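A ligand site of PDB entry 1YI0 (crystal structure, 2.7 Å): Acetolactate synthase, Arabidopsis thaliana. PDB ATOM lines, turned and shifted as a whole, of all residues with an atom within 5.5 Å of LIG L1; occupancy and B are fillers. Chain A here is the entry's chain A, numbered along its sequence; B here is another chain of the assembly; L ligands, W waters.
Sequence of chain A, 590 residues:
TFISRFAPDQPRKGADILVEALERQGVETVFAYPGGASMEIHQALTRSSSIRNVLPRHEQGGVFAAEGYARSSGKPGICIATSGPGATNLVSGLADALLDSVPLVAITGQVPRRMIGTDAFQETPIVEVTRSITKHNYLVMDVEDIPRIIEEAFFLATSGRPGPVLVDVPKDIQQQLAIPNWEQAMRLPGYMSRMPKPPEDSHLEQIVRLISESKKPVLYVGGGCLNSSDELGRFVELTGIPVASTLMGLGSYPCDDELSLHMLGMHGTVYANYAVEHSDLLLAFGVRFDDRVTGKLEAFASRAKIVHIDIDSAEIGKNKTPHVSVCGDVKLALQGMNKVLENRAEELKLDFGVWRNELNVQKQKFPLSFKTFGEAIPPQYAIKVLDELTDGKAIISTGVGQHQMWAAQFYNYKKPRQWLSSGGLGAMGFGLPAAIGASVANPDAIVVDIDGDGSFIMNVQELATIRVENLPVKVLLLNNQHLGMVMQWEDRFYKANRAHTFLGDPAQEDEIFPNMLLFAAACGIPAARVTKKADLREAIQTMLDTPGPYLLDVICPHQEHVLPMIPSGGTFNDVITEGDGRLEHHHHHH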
ATOM      1  N   MET A 266      14.261  17.479 -15.954  1.00  0.00           N
ATOM      2  CA  MET A 266      15.026  18.708 -15.806  1.00  0.00           C
ATOM      3  C   MET A 266      16.507  18.477 -15.529  1.00  0.00           C
ATOM      4  O   MET A 266      17.378  19.065 -16.186  1.00  0.00           O
ATOM      5  CB  MET A 266      14.411  19.559 -14.684  1.00  0.00           C
ATOM      6  CG  MET A 266      15.148  20.851 -14.397  1.00  0.00           C
ATOM      7  SD  MET A 266      14.139  21.951 -13.399  1.00  0.00           S
ATOM      8  CE  MET A 266      13.010  22.537 -14.641  1.00  0.00           C
ATOM      9  N   HIS A 267      16.789  17.607 -14.571  1.00  0.00           N
ATOM     10  CA  HIS A 267      18.153  17.289 -14.207  1.00  0.00           C
ATOM     11  C   HIS A 267      18.472  15.846 -14.543  1.00  0.00           C
ATOM     12  O   HIS A 267      19.334  15.220 -13.921  1.00  0.00           O
ATOM     13  CB  HIS A 267      18.366  17.550 -12.722  1.00  0.00           C
ATOM     14  CG  HIS A 267      18.244  18.997 -12.346  1.00  0.00           C
ATOM     15  ND1 HIS A 267      19.117  19.967 -12.794  1.00  0.00           N
ATOM     16  CD2 HIS A 267      17.335  19.645 -11.580  1.00  0.00           C
ATOM     17  CE1 HIS A 267      18.764  21.140 -12.314  1.00  0.00           C
ATOM     18  NE2 HIS A 267      17.683  20.979 -11.571  1.00  0.00           N
ATOM     19  N   ASP A 291       5.696  18.342 -15.026  1.00  0.00           N
ATOM     20  CA  ASP A 291       6.436  19.359 -15.784  1.00  0.00           C
ATOM     21  C   ASP A 291       7.955  19.196 -15.624  1.00  0.00           C
ATOM     22  O   ASP A 291       8.719  19.558 -16.525  1.00  0.00           O
ATOM     23  CB  ASP A 291       5.992  20.777 -15.387  1.00  0.00           C
ATOM     24  CG  ASP A 291       6.340  21.137 -13.937  1.00  0.00           C
ATOM     25  OD1 ASP A 291       5.518  20.914 -13.022  1.00  0.00           O
ATOM     26  OD2 ASP A 291       7.462  21.656 -13.733  1.00  0.00           O
ATOM     27  N   ARG A 292       8.386  18.665 -14.481  1.00  0.00           N
ATOM     28  CA  ARG A 292       9.810  18.443 -14.221  1.00  0.00           C
ATOM     29  C   ARG A 292      10.415  17.474 -15.241  1.00  0.00           C
ATOM     30  O   ARG A 292      11.571  17.597 -15.610  1.00  0.00           O
ATOM     31  CB  ARG A 292      10.009  17.871 -12.823  1.00  0.00           C
ATOM     32  CG  ARG A 292      10.391  18.898 -11.791  1.00  0.00           C
ATOM     33  CD  ARG A 292       9.678  20.190 -12.056  1.00  0.00           C
ATOM     34  NE  ARG A 292      10.577  21.303 -11.839  1.00  0.00           N
ATOM     35  CZ  ARG A 292      10.327  22.573 -12.144  1.00  0.00           C
ATOM     36  NH1 ARG A 292       9.164  22.913 -12.696  1.00  0.00           N
ATOM     37  NH2 ARG A 292      11.237  23.497 -11.882  1.00  0.00           N
ATOM     38  N   MET A 485      20.344  25.304  -4.644  1.00  0.00           N
ATOM     39  CA  MET A 485      19.478  25.302  -5.806  1.00  0.00           C
ATOM     40  C   MET A 485      19.042  26.720  -6.200  1.00  0.00           C
ATOM     41  O   MET A 485      19.050  27.062  -7.382  1.00  0.00           O
ATOM     42  CB  MET A 485      18.244  24.425  -5.532  1.00  0.00           C
ATOM     43  CG  MET A 485      17.402  24.124  -6.756  1.00  0.00           C
ATOM     44  SD  MET A 485      18.348  23.422  -8.123  1.00  0.00           S
ATOM     45  CE  MET A 485      18.251  21.679  -7.740  1.00  0.00           C
ATOM     46  N   VAL A 486      18.685  27.535  -5.222  1.00  0.00           N
ATOM     47  CA  VAL A 486      18.269  28.904  -5.528  1.00  0.00           C
ATOM     48  C   VAL A 486      19.444  29.752  -6.020  1.00  0.00           C
ATOM     49  O   VAL A 486      19.262  30.564  -6.929  1.00  0.00           O
ATOM     50  CB  VAL A 486      17.622  29.610  -4.319  1.00  0.00           C
ATOM     51  CG1 VAL A 486      17.156  30.999  -4.717  1.00  0.00           C
ATOM     52  CG2 VAL A 486      16.456  28.798  -3.826  1.00  0.00           C
ATOM     53  N   TRP A 489      20.091  29.199  -9.623  1.00  0.00           N
ATOM     54  CA  TRP A 489      19.167  29.929 -10.475  1.00  0.00           C
ATOM     55  C   TRP A 489      19.533  31.415 -10.486  1.00  0.00           C
ATOM     56  O   TRP A 489      19.310  32.104 -11.490  1.00  0.00           O
ATOM     57  CB  TRP A 489      17.713  29.687 -10.017  1.00  0.00           C
ATOM     58  CG  TRP A 489      17.119  28.402 -10.586  1.00  0.00           C
ATOM     59  CD1 TRP A 489      17.615  27.127 -10.455  1.00  0.00           C
ATOM     60  CD2 TRP A 489      15.927  28.283 -11.391  1.00  0.00           C
ATOM     61  NE1 TRP A 489      16.812  26.232 -11.125  1.00  0.00           N
ATOM     62  CE2 TRP A 489      15.772  26.911 -11.703  1.00  0.00           C
ATOM     63  CE3 TRP A 489      14.979  29.199 -11.862  1.00  0.00           C
ATOM     64  CZ2 TRP A 489      14.700  26.436 -12.485  1.00  0.00           C
ATOM     65  CZ3 TRP A 489      13.921  28.727 -12.640  1.00  0.00           C
ATOM     66  CH2 TRP A 489      13.792  27.359 -12.945  1.00  0.00           C
ATOM     67  N   SER A 568      13.008  25.333 -17.312  1.00  0.00           N
ATOM     68  CA  SER A 568      11.572  25.120 -17.233  1.00  0.00           C
ATOM     69  C   SER A 568      10.821  25.347 -18.541  1.00  0.00           C
ATOM     70  O   SER A 568      11.036  26.363 -19.212  1.00  0.00           O
ATOM     71  CB  SER A 568      10.962  26.010 -16.153  1.00  0.00           C
ATOM     72  OG  SER A 568      11.284  25.525 -14.865  1.00  0.00           O
ATOM     73  N   GLY A 569       9.942  24.411 -18.875  1.00  0.00           N
ATOM     74  CA  GLY A 569       9.158  24.511 -20.096  1.00  0.00           C
ATOM     75  C   GLY A 569      10.028  24.438 -21.335  1.00  0.00           C
ATOM     76  O   GLY A 569       9.612  24.823 -22.423  1.00  0.00           O
ATOM     77  N   GLY B  35      12.513  31.048  -2.342  1.00  0.00           N
ATOM     78  CA  GLY B  35      12.152  29.779  -2.931  1.00  0.00           C
ATOM     79  C   GLY B  35      11.925  30.007  -4.419  1.00  0.00           C
ATOM     80  O   GLY B  35      11.829  31.163  -4.850  1.00  0.00           O
ATOM     81  N   GLY B  36      11.835  28.940  -5.201  1.00  0.00           N
ATOM     82  CA  GLY B  36      11.639  29.066  -6.635  1.00  0.00           C
ATOM     83  C   GLY B  36      10.538  30.020  -7.067  1.00  0.00           C
ATOM     84  O   GLY B  36      10.788  30.990  -7.808  1.00  0.00           O
ATOM     85  N   ALA B  37       9.322  29.773  -6.598  1.00  0.00           N
ATOM     86  CA  ALA B  37       8.178  30.603  -6.963  1.00  0.00           C
ATOM     87  C   ALA B  37       8.265  32.057  -6.490  1.00  0.00           C
ATOM     88  O   ALA B  37       7.469  32.887  -6.923  1.00  0.00           O
ATOM     89  CB  ALA B  37       6.898  29.964  -6.440  1.00  0.00           C
ATOM     90  N   MET B  39      11.490  33.883  -6.261  1.00  0.00           N
ATOM     91  CA  MET B  39      12.775  34.495  -6.586  1.00  0.00           C
ATOM     92  C   MET B  39      12.665  35.940  -7.037  1.00  0.00           C
ATOM     93  O   MET B  39      13.409  36.806  -6.583  1.00  0.00           O
ATOM     94  CB  MET B  39      13.501  33.682  -7.650  1.00  0.00           C
ATOM     95  CG  MET B  39      14.047  32.382  -7.140  1.00  0.00           C
ATOM     96  SD  MET B  39      15.168  31.637  -8.318  1.00  0.00           S
ATOM     97  CE  MET B  39      16.695  32.527  -7.925  1.00  0.00           C
ATOM     98  N   THR B  82       7.834  31.128  -0.371  1.00  0.00           N
ATOM     99  CA  THR B  82       7.695  30.641  -1.726  1.00  0.00           C
ATOM    100  C   THR B  82       6.428  29.778  -1.773  1.00  0.00           C
ATOM    101  O   THR B  82       5.673  29.726  -0.804  1.00  0.00           O
ATOM    102  CB  THR B  82       8.933  29.834  -2.172  1.00  0.00           C
ATOM    103  OG1 THR B  82       8.843  29.533  -3.573  1.00  0.00           O
ATOM    104  CG2 THR B  82       9.031  28.545  -1.392  1.00  0.00           C
ATOM    105  N   SER B  83       6.203  29.108  -2.885  1.00  0.00           N
ATOM    106  CA  SER B  83       5.016  28.280  -3.020  1.00  0.00           C
ATOM    107  C   SER B  83       5.153  26.938  -2.317  1.00  0.00           C
ATOM    108  O   SER B  83       6.159  26.681  -1.656  1.00  0.00           O
ATOM    109  CB  SER B  83       4.698  28.057  -4.499  1.00  0.00           C
ATOM    110  OG  SER B  83       5.718  27.333  -5.145  1.00  0.00           O
ATOM    111  N   GLN B 110       3.462  31.694  -6.050  1.00  0.00           N
ATOM    112  CA  GLN B 110       2.662  30.603  -6.591  1.00  0.00           C
ATOM    113  C   GLN B 110       3.265  30.217  -7.910  1.00  0.00           C
ATOM    114  O   GLN B 110       4.062  30.957  -8.478  1.00  0.00           O
ATOM    115  CB  GLN B 110       1.222  31.051  -6.849  1.00  0.00           C
ATOM    116  CG  GLN B 110       0.165  30.335  -6.048  1.00  0.00           C
ATOM    117  CD  GLN B 110       0.216  28.810  -6.137  1.00  0.00           C
ATOM    118  OE1 GLN B 110      -0.590  28.139  -5.480  1.00  0.00           O
ATOM    119  NE2 GLN B 110       1.127  28.271  -6.922  1.00  0.00           N
ATOM    120  N   VAL B 111       2.855  29.057  -8.419  1.00  0.00           N
ATOM    121  CA  VAL B 111       3.314  28.593  -9.711  1.00  0.00           C
ATOM    122  C   VAL B 111       2.607  29.483 -10.732  1.00  0.00           C
ATOM    123  O   VAL B 111       1.640  30.176 -10.402  1.00  0.00           O
ATOM    124  CB  VAL B 111       2.905  27.120  -9.918  1.00  0.00           C
ATOM    125  CG1 VAL B 111       3.513  26.273  -8.813  1.00  0.00           C
ATOM    126  CG2 VAL B 111       1.381  26.989  -9.914  1.00  0.00           C
ATOM    127  N   PRO B 112       3.081  29.491 -11.989  1.00  0.00           N
ATOM    128  CA  PRO B 112       2.444  30.322 -13.013  1.00  0.00           C
ATOM    129  C   PRO B 112       0.946  30.006 -13.120  1.00  0.00           C
ATOM    130  O   PRO B 112       0.540  28.863 -12.967  1.00  0.00           O
ATOM    131  CB  PRO B 112       3.204  29.950 -14.290  1.00  0.00           C
ATOM    132  CG  PRO B 112       4.579  29.622 -13.752  1.00  0.00           C
ATOM    133  CD  PRO B 112       4.265  28.800 -12.522  1.00  0.00           C
ATOM    134  N   MET B 115      -0.373  27.016 -14.747  1.00  0.00           N
ATOM    135  CA  MET B 115       0.050  25.778 -14.084  1.00  0.00           C
ATOM    136  C   MET B 115      -0.839  25.424 -12.893  1.00  0.00           C
ATOM    137  O   MET B 115      -0.805  24.298 -12.391  1.00  0.00           O
ATOM    138  CB  MET B 115       1.493  25.903 -13.580  1.00  0.00           C
ATOM    139  CG  MET B 115       2.562  25.994 -14.648  1.00  0.00           C
ATOM    140  SD  MET B 115       2.648  24.502 -15.610  1.00  0.00           S
ATOM    141  CE  MET B 115       2.522  25.201 -17.279  1.00  0.00           C
ATOM    142  N   ALA B 120       1.136  20.866 -10.311  1.00  0.00           N
ATOM    143  CA  ALA B 120       2.443  21.364 -10.725  1.00  0.00           C
ATOM    144  C   ALA B 120       3.497  21.278  -9.641  1.00  0.00           C
ATOM    145  O   ALA B 120       3.194  21.097  -8.457  1.00  0.00           O
ATOM    146  CB  ALA B 120       2.324  22.805 -11.217  1.00  0.00           C
ATOM    147  N   PHE B 121       4.755  21.412 -10.057  1.00  0.00           N
ATOM    148  CA  PHE B 121       5.880  21.371  -9.140  1.00  0.00           C
ATOM    149  C   PHE B 121       5.708  22.409  -8.031  1.00  0.00           C
ATOM    150  O   PHE B 121       5.574  23.599  -8.304  1.00  0.00           O
ATOM    151  CB  PHE B 121       7.173  21.645  -9.907  1.00  0.00           C
ATOM    152  CG  PHE B 121       8.391  21.725  -9.046  1.00  0.00           C
ATOM    153  CD1 PHE B 121       8.773  20.647  -8.259  1.00  0.00           C
ATOM    154  CD2 PHE B 121       9.182  22.878  -9.042  1.00  0.00           C
ATOM    155  CE1 PHE B 121       9.929  20.707  -7.476  1.00  0.00           C
ATOM    156  CE2 PHE B 121      10.345  22.944  -8.261  1.00  0.00           C
ATOM    157  CZ  PHE B 121      10.706  21.858  -7.475  1.00  0.00           C
ATOM    158  N   GLN B 122       5.714  21.938  -6.795  1.00  0.00           N
ATOM    159  CA  GLN B 122       5.582  22.805  -5.628  1.00  0.00           C
ATOM    160  C   GLN B 122       4.335  23.688  -5.595  1.00  0.00           C
ATOM    161  O   GLN B 122       4.424  24.867  -5.226  1.00  0.00           O
ATOM    162  CB  GLN B 122       6.800  23.709  -5.486  1.00  0.00           C
ATOM    163  CG  GLN B 122       8.111  22.981  -5.439  1.00  0.00           C
ATOM    164  CD  GLN B 122       9.182  23.791  -4.721  1.00  0.00           C
ATOM    165  OE1 GLN B 122       9.537  24.890  -5.156  1.00  0.00           O
ATOM    166  NE2 GLN B 122       9.677  23.254  -3.614  1.00  0.00           N
ATOM    167  N   LYS B 171       3.890  33.222 -10.143  1.00  0.00           N
ATOM    168  CA  LYS B 171       5.206  33.594 -10.641  1.00  0.00           C
ATOM    169  C   LYS B 171       5.189  34.362 -11.956  1.00  0.00           C
ATOM    170  O   LYS B 171       5.995  35.281 -12.150  1.00  0.00           O
ATOM    171  CB  LYS B 171       6.082  32.351 -10.776  1.00  0.00           C
ATOM    172  CG  LYS B 171       7.531  32.697 -11.076  1.00  0.00           C
ATOM    173  CD  LYS B 171       8.414  31.483 -11.231  1.00  0.00           C
ATOM    174  CE  LYS B 171       9.790  31.906 -11.704  1.00  0.00           C
ATOM    175  NZ  LYS B 171      10.701  30.766 -11.946  1.00  0.00           N
HETATM  176  C1  LIG L   1       6.004  24.605 -13.731  1.00  0.00           C
HETATM  177  C2  LIG L   1       5.446  24.174 -12.405  1.00  0.00           C
HETATM  178  C3  LIG L   1       5.830  24.929 -11.170  1.00  0.00           C
HETATM  179  C4  LIG L   1       6.780  26.118 -11.221  1.00  0.00           C
HETATM  180  C5  LIG L   1       7.326  26.512 -12.563  1.00  0.00           C
HETATM  181  C6  LIG L   1       6.937  25.754 -13.825  1.00  0.00           C
HETATM  182  S1  LIG L   1       8.470  27.834 -13.067  1.00  0.00           S
HETATM  183  N1  LIG L   1       9.714  28.006 -11.864  1.00  0.00           N
HETATM  184  C7  LIG L   1      10.530  26.999 -11.499  1.00  0.00           C
HETATM  185  N2  LIG L   1      11.474  27.235 -10.583  1.00  0.00           N
HETATM  186  C8  LIG L   1      12.462  26.661  -9.907  1.00  0.00           C
HETATM  187  N3  LIG L   1      12.629  25.300 -10.158  1.00  0.00           N
HETATM  188  C9  LIG L   1      13.631  24.578  -9.522  1.00  0.00           C
HETATM  189  C10 LIG L   1      14.583  25.219  -8.532  1.00  0.00           C
HETATM  190  C11 LIG L   1      14.317  26.679  -8.335  1.00  0.00           C
HETATM  191  N4  LIG L   1      13.269  27.372  -9.023  1.00  0.00           N
HETATM  192  O1  LIG L   1       9.217  27.380 -14.406  1.00  0.00           O
HETATM  193  O2  LIG L   1       7.868  29.201 -12.994  1.00  0.00           O
HETATM  194  O3  LIG L   1      10.405  25.881 -12.012  1.00  0.00           O
HETATM  195  C12 LIG L   1       7.266  26.969 -10.086  1.00  0.00           C
HETATM  196  O4  LIG L   1       8.331  26.450  -9.274  1.00  0.00           O
HETATM  197  C13 LIG L   1       8.017  26.265  -7.876  1.00  0.00           C
HETATM  198  O5  LIG L   1       6.768  28.083  -9.916  1.00  0.00           O
HETATM  199  C14 LIG L   1      15.118  27.395  -7.456  1.00  0.00           C
HETATM  200  C15 LIG L   1      13.773  23.243  -9.776  1.00  0.00           C
HETATM  201  P1  LG2 L   2       4.593  10.012  -8.569  1.00  0.00           P
HETATM  202  O1  LG2 L   2       4.751   9.226  -7.314  1.00  0.00           O
HETATM  203  O2  LG2 L   2       4.492  11.439  -8.531  1.00  0.00           O
HETATM  204  O3  LG2 L   2       3.423   9.568  -9.390  1.00  0.00           O
HETATM  205  C1  LG2 L   2       3.176   8.133  -9.557  1.00  0.00           C
HETATM  206  C2  LG2 L   2       2.019   7.935 -10.486  1.00  0.00           C
HETATM  207  O4  LG2 L   2       1.862   6.533 -10.547  1.00  0.00           O
HETATM  208  C3  LG2 L   2       0.546   8.496 -10.215  1.00  0.00           C
HETATM  209  O5  LG2 L   2      -0.123   9.029 -11.340  1.00  0.00           O
HETATM  210  C4  LG2 L   2      -0.089   7.332  -9.525  1.00  0.00           C
HETATM  211  O6  LG2 L   2      -1.425   7.345  -9.179  1.00  0.00           O
HETATM  212  C5  LG2 L   2       0.496   6.202 -10.385  1.00  0.00           C
HETATM  213  N1  LG2 L   2       0.481   4.797  -9.763  1.00  0.00           N
HETATM  214  C6  LG2 L   2       0.673   4.608  -8.308  1.00  0.00           C
HETATM  215  N2  LG2 L   2       0.637   3.379  -7.889  1.00  0.00           N
HETATM  216  C7  LG2 L   2       0.416   2.645  -9.003  1.00  0.00           C
HETATM  217  C8  LG2 L   2       0.229   1.147  -9.390  1.00  0.00           C
HETATM  218  N3  LG2 L   2       0.301   0.202  -8.464  1.00  0.00           N
HETATM  219  N4  LG2 L   2      -0.010   0.783 -10.778  1.00  0.00           N
HETATM  220  C9  LG2 L   2      -0.095   1.776 -11.816  1.00  0.00           C
HETATM  221  N5  LG2 L   2       0.059   3.155 -11.577  1.00  0.00           N
HETATM  222  C10 LG2 L   2       0.306   3.544 -10.178  1.00  0.00           C
HETATM  223  N6  LG2 L   2      11.772  14.444 -11.307  1.00  0.00           N
HETATM  224  C11 LG2 L   2      12.336  13.927 -12.392  1.00  0.00           C
HETATM  225  O7  LG2 L   2      11.939  12.821 -12.749  1.00  0.00           O
HETATM  226  N7  LG2 L   2      13.410  14.574 -13.037  1.00  0.00           N
HETATM  227  C12 LG2 L   2      13.976  15.773 -12.547  1.00  0.00           C
HETATM  228  O8  LG2 L   2      14.852  16.399 -13.165  1.00  0.00           O
HETATM  229  C13 LG2 L   2      13.414  16.301 -11.295  1.00  0.00           C
HETATM  230  N8  LG2 L   2      13.952  17.437 -10.727  1.00  0.00           N
HETATM  231  C14 LG2 L   2      13.437  17.881  -9.536  1.00  0.00           C
HETATM  232  C15 LG2 L   2      14.124  18.951  -8.879  1.00  0.00           C
HETATM  233  C16 LG2 L   2      13.758  19.343  -7.557  1.00  0.00           C
HETATM  234  C17 LG2 L   2      14.631  20.339  -6.855  1.00  0.00           C
HETATM  235  C18 LG2 L   2      12.622  18.676  -6.896  1.00  0.00           C
HETATM  236  C19 LG2 L   2      12.239  18.952  -5.449  1.00  0.00           C
HETATM  237  C20 LG2 L   2      11.882  17.677  -7.592  1.00  0.00           C
HETATM  238  C21 LG2 L   2      12.287  17.211  -8.879  1.00  0.00           C
HETATM  239  N9  LG2 L   2      11.663  16.125  -9.564  1.00  0.00           N
HETATM  240  C22 LG2 L   2      12.257  15.596 -10.721  1.00  0.00           C
HETATM  241  C23 LG2 L   2      10.590  15.300  -8.872  1.00  0.00           C
HETATM  242  C24 LG2 L   2       9.332  15.737  -9.514  1.00  0.00           C
HETATM  243  O9  LG2 L   2       8.776  16.913  -8.906  1.00  0.00           O
HETATM  244  C25 LG2 L   2       8.157  14.729  -9.487  1.00  0.00           C
HETATM  245  O10 LG2 L   2       7.969  14.410  -8.010  1.00  0.00           O
HETATM  246  C26 LG2 L   2       8.415  13.332 -10.127  1.00  0.00           C
HETATM  247  O11 LG2 L   2       8.854  13.597 -11.562  1.00  0.00           O
HETATM  248  C27 LG2 L   2       7.158  12.568 -10.114  1.00  0.00           C
HETATM  249  O12 LG2 L   2       7.458  11.284 -10.731  1.00  0.00           O
HETATM  250  P2  LG2 L   2       6.385  10.178 -10.893  1.00  0.00           P
HETATM  251  O13 LG2 L   2       5.294  10.780 -11.715  1.00  0.00           O
HETATM  252  O14 LG2 L   2       7.049   9.097 -11.543  1.00  0.00           O
HETATM  253  O15 LG2 L   2       5.892   9.659  -9.456  1.00  0.00           O
HETATM  254  O   HOH W   1      16.779  23.549 -11.208  1.00  0.00           O
HETATM  255  O   HOH W   2       6.879  30.903 -15.571  1.00  0.00           O
HETATM  256  O   HOH W   3      12.422  30.033  -9.944  1.00  0.00           O
HETATM  257  O   HOH W   4       8.416  27.379  -4.821  1.00  0.00           O
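An oxygen (O3) of LIG L1 sits at hydrogen-bond distance from the guanidinium group (NH2) of Arg 292 (2.5 Å).
The side-chain hydroxyl (OG) of Ser 568 is in hydrogen-bond range of an oxygen (O1) of LIG L1 (2.8 Å).
A nitrogen (N1) of LIG L1 lies within hydrogen-bond range of the side-chain amino group (NZ) of Lys 171 of chain B, at 2.9 Å.
N of Met 266 lies within hydrogen-bond range of O8 of LG2 L2 (3.0 Å).
N of His 267 is in hydrogen-bond range of O8 of LG2 L2.
Residues that only touch LIG L1: Met 266 (3.9 Å), Asp 291 (3.3 Å), Met 485 (3.5 Å), Val 486 (3.99 Å), Trp 489 (3.3 Å), Gly 36 of chain B (3.4 Å), Ala 37 of chain B (3.95 Å), Ser 83 of chain B (3.7 Å), Val 111 of chain B (3.5 Å), Pro 112 of chain B (3.4 Å), Met 115 of chain B (3.8 Å), Ala 120 of chain B (3.6 Å), Phe 121 of chain B (3.2 Å) and Gln 122 of chain B (3.4 Å).
Hydrophobic or aromatic side chains within 4 Å of LIG L1: Met 266, Met 485, Trp 489, Ala 37 of chain B, Val 111 of chain B, Pro 112 of chain B, Met 115 of chain B, Ala 120 of chain B and Phe 121 of chain B.
17 residues have an atom within 4 Å of LIG L1: Met 266, Asp 291, Arg 292, Met 485, Val 486, Trp 489, Ser 568, Gly 36 of chain B, Ala 37 of chain B, Ser 83 of chain B, Val 111 of chain B, Pro 112 of chain B, Met 115 of chain B, Ala 120 of chain B, Phe 121 of chain B, Gln 122 of chain B and Lys 171 of chain B.
The nearest printed residue that does not touch LIG L1 is Gln 110 of chain B (4.2 Å).
Water W4 lies within hydrogen-bond range of OG1 of Thr 82 of chain B (2.5 Å), OG of Ser 83 of chain B (2.7 Å), OE1 of Gln 122 of chain B (2.8 Å) and N of Ala 37 of chain B (3.1 Å).
Water W1 lies within hydrogen-bond range of the indole nitrogen of Trp 489 (2.7 Å), a ring nitrogen (NE2) of His 267 (2.7 Å), the side-chain sulfur of Met 485 (3.5 Å) and the side-chain sulfur of Met 266 (3.8 Å).
The side-chain carboxylate of Asp 291 lies within salt-bridge range of the guanidinium group of Arg 292, 3.7 Å away.
The backbone NH of Met 266 sits at hydrogen-bond distance from the backbone carbonyl oxygen of Arg 292 (2.7 Å).
N of Phe 121 of chain B sits at hydrogen-bond distance from OD1 of Asp 291, 3.1 Å away.
The side-chain hydroxyl (OG1) of Thr 82 of chain B sits at hydrogen-bond distance from the backbone NH (N) of Gly 36 of chain B, at 3.5 Å.
O of Gln 122 of chain B sits at hydrogen-bond distance from OG of Ser 83 of chain B (2.8 Å).
N of Ala 37 of chain B lies within hydrogen-bond range of OG1 of Thr 82 of chain B (3.1 Å).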
